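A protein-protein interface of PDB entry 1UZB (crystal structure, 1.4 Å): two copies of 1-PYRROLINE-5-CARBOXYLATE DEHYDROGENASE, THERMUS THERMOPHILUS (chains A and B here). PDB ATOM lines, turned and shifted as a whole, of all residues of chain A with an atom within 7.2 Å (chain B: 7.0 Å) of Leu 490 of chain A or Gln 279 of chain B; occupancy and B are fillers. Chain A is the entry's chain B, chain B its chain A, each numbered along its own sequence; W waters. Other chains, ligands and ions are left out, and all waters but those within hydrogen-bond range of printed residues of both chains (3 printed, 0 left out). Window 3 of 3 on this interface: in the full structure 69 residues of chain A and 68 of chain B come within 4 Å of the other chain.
O of Lys 283 of chain B sits at hydrogen-bond distance from OH of Tyr 269 of chain A, 2.7 Å away. The backbone NH (N) of Leu 490 of chain A lies within hydrogen-bond range of the backbone carbonyl oxygen (O) of Thr 280 of chain B, at 3.4 Å.
O of Trp 281 of chain B sits at hydrogen-bond distance from NE2 of Gln 279 of chain B (2.9 Å). The backbone NH (N) of Thr 289 of chain A is in hydrogen-bond range of the backbone carbonyl oxygen (O) of Ser 491 of chain A, 2.9 Å away. The side-chain amino group (NZ) of Lys 489 of chain A sits at hydrogen-bond distance from the backbone carbonyl oxygen (O) of Thr 441 of chain A, 2.8 Å away. The backbone carbonyl oxygen (O) of Val 248 of chain B lies within hydrogen-bond range of the side-chain amino group (NZ) of Lys 283 of chain B, 2.8 Å away. The side-chain hydroxyl of Thr 289 of chain A lies within hydrogen-bond range of the backbone carbonyl oxygen of Leu 490 of chain A, 2.7 Å away.
Phe 282 of chain B touches Leu 262 of chain A. Leu 266 of chain A touches Phe 282 of chain B (CD2 to CE2, 3.9 Å). Ala 272 of chain B touches Tyr 269 of chain A (O to CE1, 3.96 Å). Gly 273 of chain B touches Tyr 269 of chain A. Phe 282 of chain B touches Val 287 of chain A (CE2 to CG2, 3.9 Å). Phe 282 of chain B touches Thr 289 of chain A (CE1 to OG1, 3.8 Å). CB of Lys 489 of chain A touches O of Thr 280 of chain B, at 3.1 Å. Lys 489 of chain A touches Trp 281 of chain B (C to CA, 3.9 Å). O of Gln 279 of chain B touches CD1 of Leu 490 of chain A, 3.99 Å away. CD2 of Leu 490 of chain A touches CE1 of Phe 282 of chain B (3.9 Å).
Printed residues of chain B within 4 Å of Leu 262 of chain A: Phe 282 (3.9 Å). Printed residues of chain B within 4 Å of Leu 266 of chain A: Leu 275 and Phe 282. Arg 274 of chain B touches none of the printed residues of chain A. No residue of chain A comes within 4 Å of Gly 278 of chain B. Of the printed residues of chain A, Gln 279 of chain B touches Leu 490 (3.99 Å). The nearest printed residue of chain B that does not touch Leu 490 of chain A is Leu 275 of chain B (4.04 Å). The nearest printed residue of chain A that does not touch Gln 279 of chain B is Pro 442 of chain A (6.1 Å).
Hydrophobic or aromatic side chains of chain A that line the printed part of chain B: Leu 262, Leu 266, Tyr 269, Val 287 and Leu 490. Of the 19 printed residues of chain B, 8 touch a printed residue of chain A. Among the printed residues, 18 pairs touch across the chains. Among the printed residues, no Asp or Glu carboxylate lies within 4 Å of a Lys or Arg side-chain nitrogen of the other chain.
No position is printed for both chains.
Water W3 lies within hydrogen-bond range of the backbone carbonyl oxygen (O) of Gly 273 of chain B and the backbone carbonyl oxygen (O) of Leu 266 of chain A. Water W2 lies within hydrogen-bond range of the backbone carbonyl oxygen of Lys 489 of chain A (2.7 Å), the backbone NH of Phe 282 of chain B (2.8 Å) and the backbone carbonyl oxygen of Gly 492 of chain A (3.0 Å). Water W1 bridges the backbone carbonyl oxygen of Lys 283 of chain B (3.2 Å) and the side-chain hydroxyl of Tyr 269 of chain A (3.3 Å).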
ATOM      1  N   SER A 261     -13.268   4.751 -20.150  1.00  0.00           N
ATOM      2  CA  SER A 261     -11.932   4.465 -19.635  1.00  0.00           C
ATOM      3  C   SER A 261     -11.630   2.977 -19.523  1.00  0.00           C
ATOM      4  O   SER A 261     -12.531   2.154 -19.353  1.00  0.00           O
ATOM      5  CB  SER A 261     -11.750   5.108 -18.260  1.00  0.00           C
ATOM      6  OG  SER A 261     -12.536   4.443 -17.287  1.00  0.00           O
ATOM      7  N   LEU A 262     -10.348   2.643 -19.598  1.00  0.00           N
ATOM      8  CA  LEU A 262      -9.914   1.258 -19.488  1.00  0.00           C
ATOM      9  C   LEU A 262     -10.264   0.695 -18.110  1.00  0.00           C
ATOM     10  O   LEU A 262     -10.692  -0.452 -17.992  1.00  0.00           O
ATOM     11  CB  LEU A 262      -8.407   1.166 -19.731  1.00  0.00           C
ATOM     12  CG  LEU A 262      -7.765  -0.208 -19.534  1.00  0.00           C
ATOM     13  CD1 LEU A 262      -8.428  -1.238 -20.450  1.00  0.00           C
ATOM     14  CD2 LEU A 262      -6.277  -0.104 -19.824  1.00  0.00           C
ATOM     15  N   LEU A 266     -12.346  -2.697 -18.013  1.00  0.00           N
ATOM     16  CA  LEU A 266     -11.832  -3.947 -17.469  1.00  0.00           C
ATOM     17  C   LEU A 266     -12.840  -4.569 -16.503  1.00  0.00           C
ATOM     18  O   LEU A 266     -13.081  -5.774 -16.536  1.00  0.00           O
ATOM     19  CB  LEU A 266     -10.499  -3.708 -16.754  1.00  0.00           C
ATOM     20  CG  LEU A 266      -9.295  -3.432 -17.662  1.00  0.00           C
ATOM     21  CD1 LEU A 266      -8.097  -3.012 -16.822  1.00  0.00           C
ATOM     22  CD2 LEU A 266      -8.962  -4.681 -18.473  1.00  0.00           C
ATOM     23  N   TYR A 269     -15.880  -5.976 -18.497  1.00  0.00           N
ATOM     24  CA  TYR A 269     -15.568  -7.222 -19.189  1.00  0.00           C
ATOM     25  C   TYR A 269     -15.483  -8.386 -18.204  1.00  0.00           C
ATOM     26  O   TYR A 269     -15.918  -9.498 -18.504  1.00  0.00           O
ATOM     27  CB  TYR A 269     -14.253  -7.082 -19.955  1.00  0.00           C
ATOM     28  CG  TYR A 269     -14.120  -8.023 -21.134  1.00  0.00           C
ATOM     29  CD1 TYR A 269     -13.189  -9.061 -21.126  1.00  0.00           C
ATOM     30  CD2 TYR A 269     -14.910  -7.855 -22.269  1.00  0.00           C
ATOM     31  CE1 TYR A 269     -13.044  -9.906 -22.230  1.00  0.00           C
ATOM     32  CE2 TYR A 269     -14.776  -8.693 -23.371  1.00  0.00           C
ATOM     33  CZ  TYR A 269     -13.841  -9.712 -23.348  1.00  0.00           C
ATOM     34  OH  TYR A 269     -13.697 -10.521 -24.454  1.00  0.00           O
ATOM     35  N   VAL A 287     -16.452  -3.399 -25.632  1.00  0.00           N
ATOM     36  CA  VAL A 287     -15.850  -2.251 -24.976  1.00  0.00           C
ATOM     37  C   VAL A 287     -14.796  -1.549 -25.824  1.00  0.00           C
ATOM     38  O   VAL A 287     -13.983  -2.193 -26.486  1.00  0.00           O
ATOM     39  CB  VAL A 287     -15.206  -2.666 -23.627  1.00  0.00           C
ATOM     40  CG1 VAL A 287     -16.239  -3.357 -22.745  1.00  0.00           C
ATOM     41  CG2 VAL A 287     -14.025  -3.589 -23.868  1.00  0.00           C
ATOM     42  N   GLU A 288     -14.845  -0.222 -25.824  1.00  0.00           N
ATOM     43  CA  GLU A 288     -13.872   0.607 -26.537  1.00  0.00           C
ATOM     44  C   GLU A 288     -13.297   1.377 -25.359  1.00  0.00           C
ATOM     45  O   GLU A 288     -14.007   2.154 -24.722  1.00  0.00           O
ATOM     46  CB  GLU A 288     -14.571   1.539 -27.529  1.00  0.00           C
ATOM     47  CG  GLU A 288     -13.634   2.245 -28.503  1.00  0.00           C
ATOM     48  CD  GLU A 288     -13.172   3.604 -28.008  1.00  0.00           C
ATOM     49  OE1 GLU A 288     -12.346   3.666 -27.073  1.00  0.00           O
ATOM     50  OE2 GLU A 288     -13.648   4.616 -28.562  1.00  0.00           O
ATOM     51  N   THR A 289     -12.016   1.160 -25.083  1.00  0.00           N
ATOM     52  CA  THR A 289     -11.373   1.731 -23.907  1.00  0.00           C
ATOM     53  C   THR A 289     -10.213   2.718 -24.042  1.00  0.00           C
ATOM     54  O   THR A 289      -9.299   2.709 -23.211  1.00  0.00           O
ATOM     55  CB  THR A 289     -10.914   0.578 -23.006  1.00  0.00           C
ATOM     56  OG1 THR A 289     -10.272  -0.417 -23.816  1.00  0.00           O
ATOM     57  CG2 THR A 289     -12.106  -0.061 -22.311  1.00  0.00           C
ATOM     58  N   GLY A 290     -10.250   3.563 -25.066  1.00  0.00           N
ATOM     59  CA  GLY A 290      -9.207   4.561 -25.243  1.00  0.00           C
ATOM     60  C   GLY A 290      -7.880   4.102 -25.817  1.00  0.00           C
ATOM     61  O   GLY A 290      -7.753   2.988 -26.323  1.00  0.00           O
ATOM     62  N   GLY A 291      -6.882   4.980 -25.743  1.00  0.00           N
ATOM     63  CA  GLY A 291      -5.567   4.652 -26.261  1.00  0.00           C
ATOM     64  C   GLY A 291      -4.490   5.644 -25.863  1.00  0.00           C
ATOM     65  O   GLY A 291      -4.734   6.573 -25.098  1.00  0.00           O
ATOM     66  N   THR A 441       3.113   0.070 -25.924  1.00  0.00           N
ATOM     67  CA  THR A 441       2.164   0.634 -24.964  1.00  0.00           C
ATOM     68  C   THR A 441       1.102  -0.454 -24.850  1.00  0.00           C
ATOM     69  O   THR A 441       1.049  -1.361 -25.681  1.00  0.00           O
ATOM     70  CB  THR A 441       1.473   1.949 -25.443  1.00  0.00           C
ATOM     71  OG1 THR A 441       0.358   1.639 -26.291  1.00  0.00           O
ATOM     72  CG2 THR A 441       2.454   2.838 -26.188  1.00  0.00           C
ATOM     73  N   PRO A 442       0.252  -0.394 -23.820  1.00  0.00           N
ATOM     74  CA  PRO A 442      -0.789  -1.415 -23.661  1.00  0.00           C
ATOM     75  C   PRO A 442      -1.954  -1.224 -24.631  1.00  0.00           C
ATOM     76  O   PRO A 442      -2.835  -2.076 -24.728  1.00  0.00           O
ATOM     77  CB  PRO A 442      -1.246  -1.226 -22.215  1.00  0.00           C
ATOM     78  CG  PRO A 442      -0.095  -0.512 -21.551  1.00  0.00           C
ATOM     79  CD  PRO A 442       0.356   0.443 -22.614  1.00  0.00           C
ATOM     80  N   TYR A 443      -1.946  -0.101 -25.345  1.00  0.00           N
ATOM     81  CA  TYR A 443      -3.029   0.237 -26.260  1.00  0.00           C
ATOM     82  C   TYR A 443      -2.767  -0.028 -27.740  1.00  0.00           C
ATOM     83  O   TYR A 443      -1.695  -0.486 -28.131  1.00  0.00           O
ATOM     84  CB  TYR A 443      -3.397   1.714 -26.081  1.00  0.00           C
ATOM     85  CG  TYR A 443      -3.933   2.074 -24.709  1.00  0.00           C
ATOM     86  CD1 TYR A 443      -3.131   2.717 -23.761  1.00  0.00           C
ATOM     87  CD2 TYR A 443      -5.261   1.813 -24.376  1.00  0.00           C
ATOM     88  CE1 TYR A 443      -3.650   3.099 -22.517  1.00  0.00           C
ATOM     89  CE2 TYR A 443      -5.787   2.187 -23.143  1.00  0.00           C
ATOM     90  CZ  TYR A 443      -4.982   2.833 -22.222  1.00  0.00           C
ATOM     91  OH  TYR A 443      -5.533   3.237 -21.027  1.00  0.00           O
ATOM     92  N   GLY A 444      -3.766   0.285 -28.560  1.00  0.00           N
ATOM     93  CA  GLY A 444      -3.648   0.092 -29.995  1.00  0.00           C
ATOM     94  C   GLY A 444      -4.853   0.632 -30.745  1.00  0.00           C
ATOM     95  O   GLY A 444      -5.434  -0.073 -31.572  1.00  0.00           O
ATOM     96  N   LEU A 445      -5.217   1.887 -30.488  1.00  0.00           N
ATOM     97  CA  LEU A 445      -6.385   2.476 -31.139  1.00  0.00           C
ATOM     98  C   LEU A 445      -6.061   3.224 -32.430  1.00  0.00           C
ATOM     99  O   LEU A 445      -6.356   2.724 -33.516  1.00  0.00           O
ATOM    100  CB  LEU A 445      -7.127   3.393 -30.159  1.00  0.00           C
ATOM    101  CG  LEU A 445      -8.501   3.889 -30.632  1.00  0.00           C
ATOM    102  CD1 LEU A 445      -9.333   2.725 -31.170  1.00  0.00           C
ATOM    103  CD2 LEU A 445      -9.225   4.566 -29.476  1.00  0.00           C
ATOM    104  N   GLY A 487     -10.121  -0.448 -31.894  1.00  0.00           N
ATOM    105  CA  GLY A 487      -8.730  -0.829 -31.753  1.00  0.00           C
ATOM    106  C   GLY A 487      -8.350  -2.240 -31.370  1.00  0.00           C
ATOM    107  O   GLY A 487      -9.170  -3.165 -31.374  1.00  0.00           O
ATOM    108  N   PHE A 488      -7.069  -2.374 -31.041  1.00  0.00           N
ATOM    109  CA  PHE A 488      -6.447  -3.628 -30.643  1.00  0.00           C
ATOM    110  C   PHE A 488      -5.987  -3.516 -29.196  1.00  0.00           C
ATOM    111  O   PHE A 488      -6.008  -2.438 -28.600  1.00  0.00           O
ATOM    112  CB  PHE A 488      -5.196  -3.900 -31.487  1.00  0.00           C
ATOM    113  CG  PHE A 488      -5.435  -3.957 -32.968  1.00  0.00           C
ATOM    114  CD1 PHE A 488      -4.422  -3.575 -33.845  1.00  0.00           C
ATOM    115  CD2 PHE A 488      -6.633  -4.427 -33.494  1.00  0.00           C
ATOM    116  CE1 PHE A 488      -4.595  -3.660 -35.225  1.00  0.00           C
ATOM    117  CE2 PHE A 488      -6.814  -4.516 -34.876  1.00  0.00           C
ATOM    118  CZ  PHE A 488      -5.790  -4.130 -35.742  1.00  0.00           C
ATOM    119  N   LYS A 489      -5.543  -4.643 -28.651  1.00  0.00           N
ATOM    120  CA  LYS A 489      -5.016  -4.689 -27.298  1.00  0.00           C
ATOM    121  C   LYS A 489      -5.928  -4.063 -26.257  1.00  0.00           C
ATOM    122  O   LYS A 489      -7.136  -4.289 -26.287  1.00  0.00           O
ATOM    123  CB  LYS A 489      -3.625  -4.052 -27.294  1.00  0.00           C
ATOM    124  CG  LYS A 489      -2.627  -4.892 -28.101  1.00  0.00           C
ATOM    125  CD  LYS A 489      -1.450  -4.096 -28.634  1.00  0.00           C
ATOM    126  CE  LYS A 489      -0.612  -3.513 -27.518  1.00  0.00           C
ATOM    127  NZ  LYS A 489       0.482  -2.669 -28.080  1.00  0.00           N
ATOM    128  N   LEU A 490      -5.380  -3.276 -25.335  1.00  0.00           N
ATOM    129  CA  LEU A 490      -6.238  -2.711 -24.304  1.00  0.00           C
ATOM    130  C   LEU A 490      -7.083  -1.520 -24.727  1.00  0.00           C
ATOM    131  O   LEU A 490      -7.650  -0.813 -23.890  1.00  0.00           O
ATOM    132  CB  LEU A 490      -5.428  -2.408 -23.038  1.00  0.00           C
ATOM    133  CG  LEU A 490      -4.926  -3.697 -22.363  1.00  0.00           C
ATOM    134  CD1 LEU A 490      -4.328  -3.378 -20.994  1.00  0.00           C
ATOM    135  CD2 LEU A 490      -6.075  -4.684 -22.209  1.00  0.00           C
ATOM    136  N   SER A 491      -7.172  -1.304 -26.036  1.00  0.00           N
ATOM    137  CA  SER A 491      -8.012  -0.246 -26.569  1.00  0.00           C
ATOM    138  C   SER A 491      -9.431  -0.798 -26.736  1.00  0.00           C
ATOM    139  O   SER A 491     -10.357  -0.065 -27.073  1.00  0.00           O
ATOM    140  CB  SER A 491      -7.473   0.256 -27.910  1.00  0.00           C
ATOM    141  OG  SER A 491      -6.342   1.083 -27.706  1.00  0.00           O
ATOM    142  N   GLY A 492      -9.607  -2.095 -26.500  1.00  0.00           N
ATOM    143  CA  GLY A 492     -10.941  -2.653 -26.605  1.00  0.00           C
ATOM    144  C   GLY A 492     -11.081  -3.995 -27.284  1.00  0.00           C
ATOM    145  O   GLY A 492     -10.100  -4.695 -27.526  1.00  0.00           O
ATOM    146  N   THR A 493     -12.325  -4.333 -27.609  1.00  0.00           N
ATOM    147  CA  THR A 493     -12.655  -5.604 -28.236  1.00  0.00           C
ATOM    148  C   THR A 493     -12.723  -5.572 -29.761  1.00  0.00           C
ATOM    149  O   THR A 493     -13.144  -6.545 -30.381  1.00  0.00           O
ATOM    150  CB  THR A 493     -13.996  -6.135 -27.690  1.00  0.00           C
ATOM    151  OG1 THR A 493     -14.980  -5.095 -27.747  1.00  0.00           O
ATOM    152  CG2 THR A 493     -13.838  -6.604 -26.251  1.00  0.00           C
ATOM    153  N   VAL B 248      -5.642 -21.218 -20.198  1.00  0.00           N
ATOM    154  CA  VAL B 248      -6.816 -20.356 -20.178  1.00  0.00           C
ATOM    155  C   VAL B 248      -6.567 -19.068 -19.391  1.00  0.00           C
ATOM    156  O   VAL B 248      -7.016 -17.994 -19.793  1.00  0.00           O
ATOM    157  CB  VAL B 248      -8.033 -21.099 -19.576  1.00  0.00           C
ATOM    158  CG1 VAL B 248      -9.147 -20.115 -19.254  1.00  0.00           C
ATOM    159  CG2 VAL B 248      -8.529 -22.156 -20.562  1.00  0.00           C
ATOM    160  N   GLU B 249      -5.841 -19.175 -18.281  1.00  0.00           N
ATOM    161  CA  GLU B 249      -5.556 -18.023 -17.425  1.00  0.00           C
ATOM    162  C   GLU B 249      -4.253 -17.293 -17.759  1.00  0.00           C
ATOM    163  O   GLU B 249      -3.935 -16.268 -17.155  1.00  0.00           O
ATOM    164  CB  GLU B 249      -5.512 -18.469 -15.959  1.00  0.00           C
ATOM    165  CG  GLU B 249      -6.776 -19.168 -15.480  1.00  0.00           C
ATOM    166  CD  GLU B 249      -6.664 -19.669 -14.051  1.00  0.00           C
ATOM    167  OE1 GLU B 249      -5.720 -20.434 -13.758  1.00  0.00           O
ATOM    168  OE2 GLU B 249      -7.525 -19.304 -13.222  1.00  0.00           O
ATOM    169  N   HIS B 250      -3.511 -17.813 -18.728  1.00  0.00           N
ATOM    170  CA  HIS B 250      -2.229 -17.235 -19.119  1.00  0.00           C
ATOM    171  C   HIS B 250      -2.365 -15.838 -19.725  1.00  0.00           C
ATOM    172  O   HIS B 250      -3.244 -15.589 -20.552  1.00  0.00           O
ATOM    173  CB  HIS B 250      -1.542 -18.172 -20.114  1.00  0.00           C
ATOM    174  CG  HIS B 250      -0.055 -18.014 -20.177  1.00  0.00           C
ATOM    175  ND1 HIS B 250       0.558 -16.869 -20.640  1.00  0.00           N
ATOM    176  CD2 HIS B 250       0.943 -18.871 -19.852  1.00  0.00           C
ATOM    177  CE1 HIS B 250       1.868 -17.027 -20.597  1.00  0.00           C
ATOM    178  NE2 HIS B 250       2.128 -18.232 -20.124  1.00  0.00           N
ATOM    179  N   PRO B 251      -1.496 -14.901 -19.319  1.00  0.00           N
ATOM    180  CA  PRO B 251      -1.591 -13.551 -19.879  1.00  0.00           C
ATOM    181  C   PRO B 251      -1.243 -13.495 -21.365  1.00  0.00           C
ATOM    182  O   PRO B 251      -1.627 -12.554 -22.058  1.00  0.00           O
ATOM    183  CB  PRO B 251      -0.607 -12.751 -19.024  1.00  0.00           C
ATOM    184  CG  PRO B 251       0.421 -13.778 -18.642  1.00  0.00           C
ATOM    185  CD  PRO B 251      -0.431 -14.978 -18.301  1.00  0.00           C
ATOM    186  N   ARG B 252      -0.535 -14.510 -21.855  1.00  0.00           N
ATOM    187  CA  ARG B 252      -0.129 -14.538 -23.257  1.00  0.00           C
ATOM    188  C   ARG B 252      -0.970 -15.419 -24.184  1.00  0.00           C
ATOM    189  O   ARG B 252      -0.576 -15.686 -25.321  1.00  0.00           O
ATOM    190  CB  ARG B 252       1.347 -14.931 -23.365  1.00  0.00           C
ATOM    191  CG  ARG B 252       2.293 -13.944 -22.697  1.00  0.00           C
ATOM    192  CD  ARG B 252       2.189 -12.561 -23.325  1.00  0.00           C
ATOM    193  NE  ARG B 252       2.550 -12.575 -24.739  1.00  0.00           N
ATOM    194  CZ  ARG B 252       2.561 -11.498 -25.520  1.00  0.00           C
ATOM    195  NH1 ARG B 252       2.231 -10.314 -25.025  1.00  0.00           N
ATOM    196  NH2 ARG B 252       2.902 -11.608 -26.798  1.00  0.00           N
ATOM    197  N   ILE B 253      -2.113 -15.888 -23.698  1.00  0.00           N
ATOM    198  CA  ILE B 253      -3.014 -16.674 -24.537  1.00  0.00           C
ATOM    199  C   ILE B 253      -4.009 -15.656 -25.095  1.00  0.00           C
ATOM    200  O   ILE B 253      -4.658 -14.924 -24.342  1.00  0.00           O
ATOM    201  CB  ILE B 253      -3.723 -17.786 -23.722  1.00  0.00           C
ATOM    202  CG1 ILE B 253      -2.856 -19.047 -23.735  1.00  0.00           C
ATOM    203  CG2 ILE B 253      -5.105 -18.082 -24.293  1.00  0.00           C
ATOM    204  CD1 ILE B 253      -2.765 -19.731 -25.100  1.00  0.00           C
ATOM    205  N   ALA B 271     -13.014 -16.913 -16.549  1.00  0.00           N
ATOM    206  CA  ALA B 271     -11.572 -16.690 -16.532  1.00  0.00           C
ATOM    207  C   ALA B 271     -11.116 -15.807 -17.693  1.00  0.00           C
ATOM    208  O   ALA B 271     -10.253 -14.944 -17.527  1.00  0.00           O
ATOM    209  CB  ALA B 271     -10.837 -18.027 -16.572  1.00  0.00           C
ATOM    210  N   ALA B 272     -11.699 -16.023 -18.869  1.00  0.00           N
ATOM    211  CA  ALA B 272     -11.341 -15.246 -20.050  1.00  0.00           C
ATOM    212  C   ALA B 272     -11.680 -13.768 -19.883  1.00  0.00           C
ATOM    213  O   ALA B 272     -11.096 -12.910 -20.549  1.00  0.00           O
ATOM    214  CB  ALA B 272     -12.054 -15.809 -21.281  1.00  0.00           C
ATOM    215  N   GLY B 273     -12.623 -13.473 -18.994  1.00  0.00           N
ATOM    216  CA  GLY B 273     -13.018 -12.094 -18.770  1.00  0.00           C
ATOM    217  C   GLY B 273     -12.081 -11.319 -17.862  1.00  0.00           C
ATOM    218  O   GLY B 273     -12.194 -10.098 -17.753  1.00  0.00           O
ATOM    219  N   ARG B 274     -11.156 -12.023 -17.215  1.00  0.00           N
ATOM    220  CA  ARG B 274     -10.209 -11.386 -16.307  1.00  0.00           C
ATOM    221  C   ARG B 274      -8.905 -11.009 -16.999  1.00  0.00           C
ATOM    222  O   ARG B 274      -8.479 -11.659 -17.956  1.00  0.00           O
ATOM    223  CB  ARG B 274      -9.890 -12.315 -15.130  1.00  0.00           C
ATOM    224  CG  ARG B 274     -11.099 -12.717 -14.301  1.00  0.00           C
ATOM    225  CD  ARG B 274     -10.681 -13.281 -12.951  1.00  0.00           C
ATOM    226  NE  ARG B 274      -9.917 -14.520 -13.066  1.00  0.00           N
ATOM    227  CZ  ARG B 274     -10.436 -15.692 -13.421  1.00  0.00           C
ATOM    228  NH1 ARG B 274      -9.660 -16.764 -13.503  1.00  0.00           N
ATOM    229  NH2 ARG B 274     -11.731 -15.795 -13.688  1.00  0.00           N
ATOM    230  N   LEU B 275      -8.274  -9.948 -16.508  1.00  0.00           N
ATOM    231  CA  LEU B 275      -7.001  -9.501 -17.052  1.00  0.00           C
ATOM    232  C   LEU B 275      -5.894 -10.108 -16.192  1.00  0.00           C
ATOM    233  O   LEU B 275      -5.664  -9.665 -15.064  1.00  0.00           O
ATOM    234  CB  LEU B 275      -6.897  -7.972 -17.007  1.00  0.00           C
ATOM    235  CG  LEU B 275      -5.667  -7.365 -17.693  1.00  0.00           C
ATOM    236  CD1 LEU B 275      -5.863  -7.383 -19.207  1.00  0.00           C
ATOM    237  CD2 LEU B 275      -5.456  -5.939 -17.206  1.00  0.00           C
ATOM    238  N   ALA B 276      -5.230 -11.136 -16.712  1.00  0.00           N
ATOM    239  CA  ALA B 276      -4.143 -11.771 -15.979  1.00  0.00           C
ATOM    240  C   ALA B 276      -3.024 -10.746 -15.847  1.00  0.00           C
ATOM    241  O   ALA B 276      -2.915  -9.831 -16.659  1.00  0.00           O
ATOM    242  CB  ALA B 276      -3.646 -12.999 -16.730  1.00  0.00           C
ATOM    243  N   PRO B 277      -2.180 -10.875 -14.814  1.00  0.00           N
ATOM    244  CA  PRO B 277      -1.087  -9.916 -14.643  1.00  0.00           C
ATOM    245  C   PRO B 277      -0.201  -9.809 -15.885  1.00  0.00           C
ATOM    246  O   PRO B 277       0.337 -10.810 -16.357  1.00  0.00           O
ATOM    247  CB  PRO B 277      -0.334 -10.469 -13.436  1.00  0.00           C
ATOM    248  CG  PRO B 277      -1.434 -11.088 -12.624  1.00  0.00           C
ATOM    249  CD  PRO B 277      -2.244 -11.811 -13.677  1.00  0.00           C
ATOM    250  N   GLY B 278      -0.062  -8.595 -16.410  1.00  0.00           N
ATOM    251  CA  GLY B 278       0.764  -8.376 -17.586  1.00  0.00           C
ATOM    252  C   GLY B 278       0.047  -8.538 -18.917  1.00  0.00           C
ATOM    253  O   GLY B 278       0.616  -8.253 -19.966  1.00  0.00           O
ATOM    254  N   GLN B 279      -1.203  -8.990 -18.876  1.00  0.00           N
ATOM    255  CA  GLN B 279      -1.992  -9.201 -20.086  1.00  0.00           C
ATOM    256  C   GLN B 279      -2.246  -7.877 -20.807  1.00  0.00           C
ATOM    257  O   GLN B 279      -2.578  -6.873 -20.176  1.00  0.00           O
ATOM    258  CB  GLN B 279      -3.310  -9.867 -19.703  1.00  0.00           C
ATOM    259  CG  GLN B 279      -4.133 -10.403 -20.856  1.00  0.00           C
ATOM    260  CD  GLN B 279      -5.342 -11.157 -20.349  1.00  0.00           C
ATOM    261  OE1 GLN B 279      -5.213 -12.064 -19.522  1.00  0.00           O
ATOM    262  NE2 GLN B 279      -6.524 -10.786 -20.830  1.00  0.00           N
ATOM    263  N   THR B 280      -2.111  -7.884 -22.132  1.00  0.00           N
ATOM    264  CA  THR B 280      -2.289  -6.667 -22.920  1.00  0.00           C
ATOM    265  C   THR B 280      -3.423  -6.700 -23.943  1.00  0.00           C
ATOM    266  O   THR B 280      -3.358  -6.033 -24.978  1.00  0.00           O
ATOM    267  CB  THR B 280      -0.987  -6.300 -23.653  1.00  0.00           C
ATOM    268  OG1 THR B 280      -0.570  -7.405 -24.461  1.00  0.00           O
ATOM    269  CG2 THR B 280       0.110  -5.965 -22.650  1.00  0.00           C
ATOM    270  N   TRP B 281      -4.463  -7.471 -23.654  1.00  0.00           N
ATOM    271  CA  TRP B 281      -5.613  -7.552 -24.544  1.00  0.00           C
ATOM    272  C   TRP B 281      -6.811  -8.138 -23.832  1.00  0.00           C
ATOM    273  O   TRP B 281      -6.696  -8.656 -22.716  1.00  0.00           O
ATOM    274  CB  TRP B 281      -5.299  -8.415 -25.776  1.00  0.00           C
ATOM    275  CG  TRP B 281      -4.767  -9.791 -25.462  1.00  0.00           C
ATOM    276  CD1 TRP B 281      -5.403 -10.795 -24.779  1.00  0.00           C
ATOM    277  CD2 TRP B 281      -3.486 -10.309 -25.833  1.00  0.00           C
ATOM    278  NE1 TRP B 281      -4.591 -11.905 -24.704  1.00  0.00           N
ATOM    279  CE2 TRP B 281      -3.409 -11.632 -25.344  1.00  0.00           C
ATOM    280  CE3 TRP B 281      -2.395  -9.783 -26.533  1.00  0.00           C
ATOM    281  CZ2 TRP B 281      -2.279 -12.437 -25.534  1.00  0.00           C
ATOM    282  CZ3 TRP B 281      -1.271 -10.585 -26.721  1.00  0.00           C
ATOM    283  CH2 TRP B 281      -1.224 -11.897 -26.223  1.00  0.00           C
ATOM    284  N   PHE B 282      -7.966  -8.032 -24.477  1.00  0.00           N
ATOM    285  CA  PHE B 282      -9.193  -8.601 -23.951  1.00  0.00           C
ATOM    286  C   PHE B 282      -9.309  -9.950 -24.657  1.00  0.00           C
ATOM    287  O   PHE B 282      -9.448 -10.016 -25.879  1.00  0.00           O
ATOM    288  CB  PHE B 282     -10.399  -7.717 -24.292  1.00  0.00           C
ATOM    289  CG  PHE B 282     -10.448  -6.429 -23.519  1.00  0.00           C
ATOM    290  CD1 PHE B 282      -9.727  -5.312 -23.934  1.00  0.00           C
ATOM    291  CD2 PHE B 282     -11.207  -6.341 -22.357  1.00  0.00           C
ATOM    292  CE1 PHE B 282      -9.762  -4.128 -23.198  1.00  0.00           C
ATOM    293  CE2 PHE B 282     -11.250  -5.166 -21.616  1.00  0.00           C
ATOM    294  CZ  PHE B 282     -10.526  -4.055 -22.034  1.00  0.00           C
ATOM    295  N   LYS B 283      -9.222 -11.027 -23.889  1.00  0.00           N
ATOM    296  CA  LYS B 283      -9.306 -12.368 -24.451  1.00  0.00           C
ATOM    297  C   LYS B 283     -10.648 -12.699 -25.077  1.00  0.00           C
ATOM    298  O   LYS B 283     -11.699 -12.271 -24.597  1.00  0.00           O
ATOM    299  CB  LYS B 283      -9.039 -13.415 -23.371  1.00  0.00           C
ATOM    300  CG  LYS B 283      -7.621 -13.475 -22.881  1.00  0.00           C
ATOM    301  CD  LYS B 283      -7.513 -14.444 -21.719  1.00  0.00           C
ATOM    302  CE  LYS B 283      -6.068 -14.650 -21.327  1.00  0.00           C
ATOM    303  NZ  LYS B 283      -5.957 -15.432 -20.066  1.00  0.00           N
HETATM  304  O   HOH W   1     -14.415 -13.651 -23.679  1.00  0.00           O
HETATM  305  O   HOH W   2      -7.979  -6.776 -27.020  1.00  0.00           O
HETATM  306  O   HOH W   3     -11.262  -7.645 -17.572  1.00  0.00           O
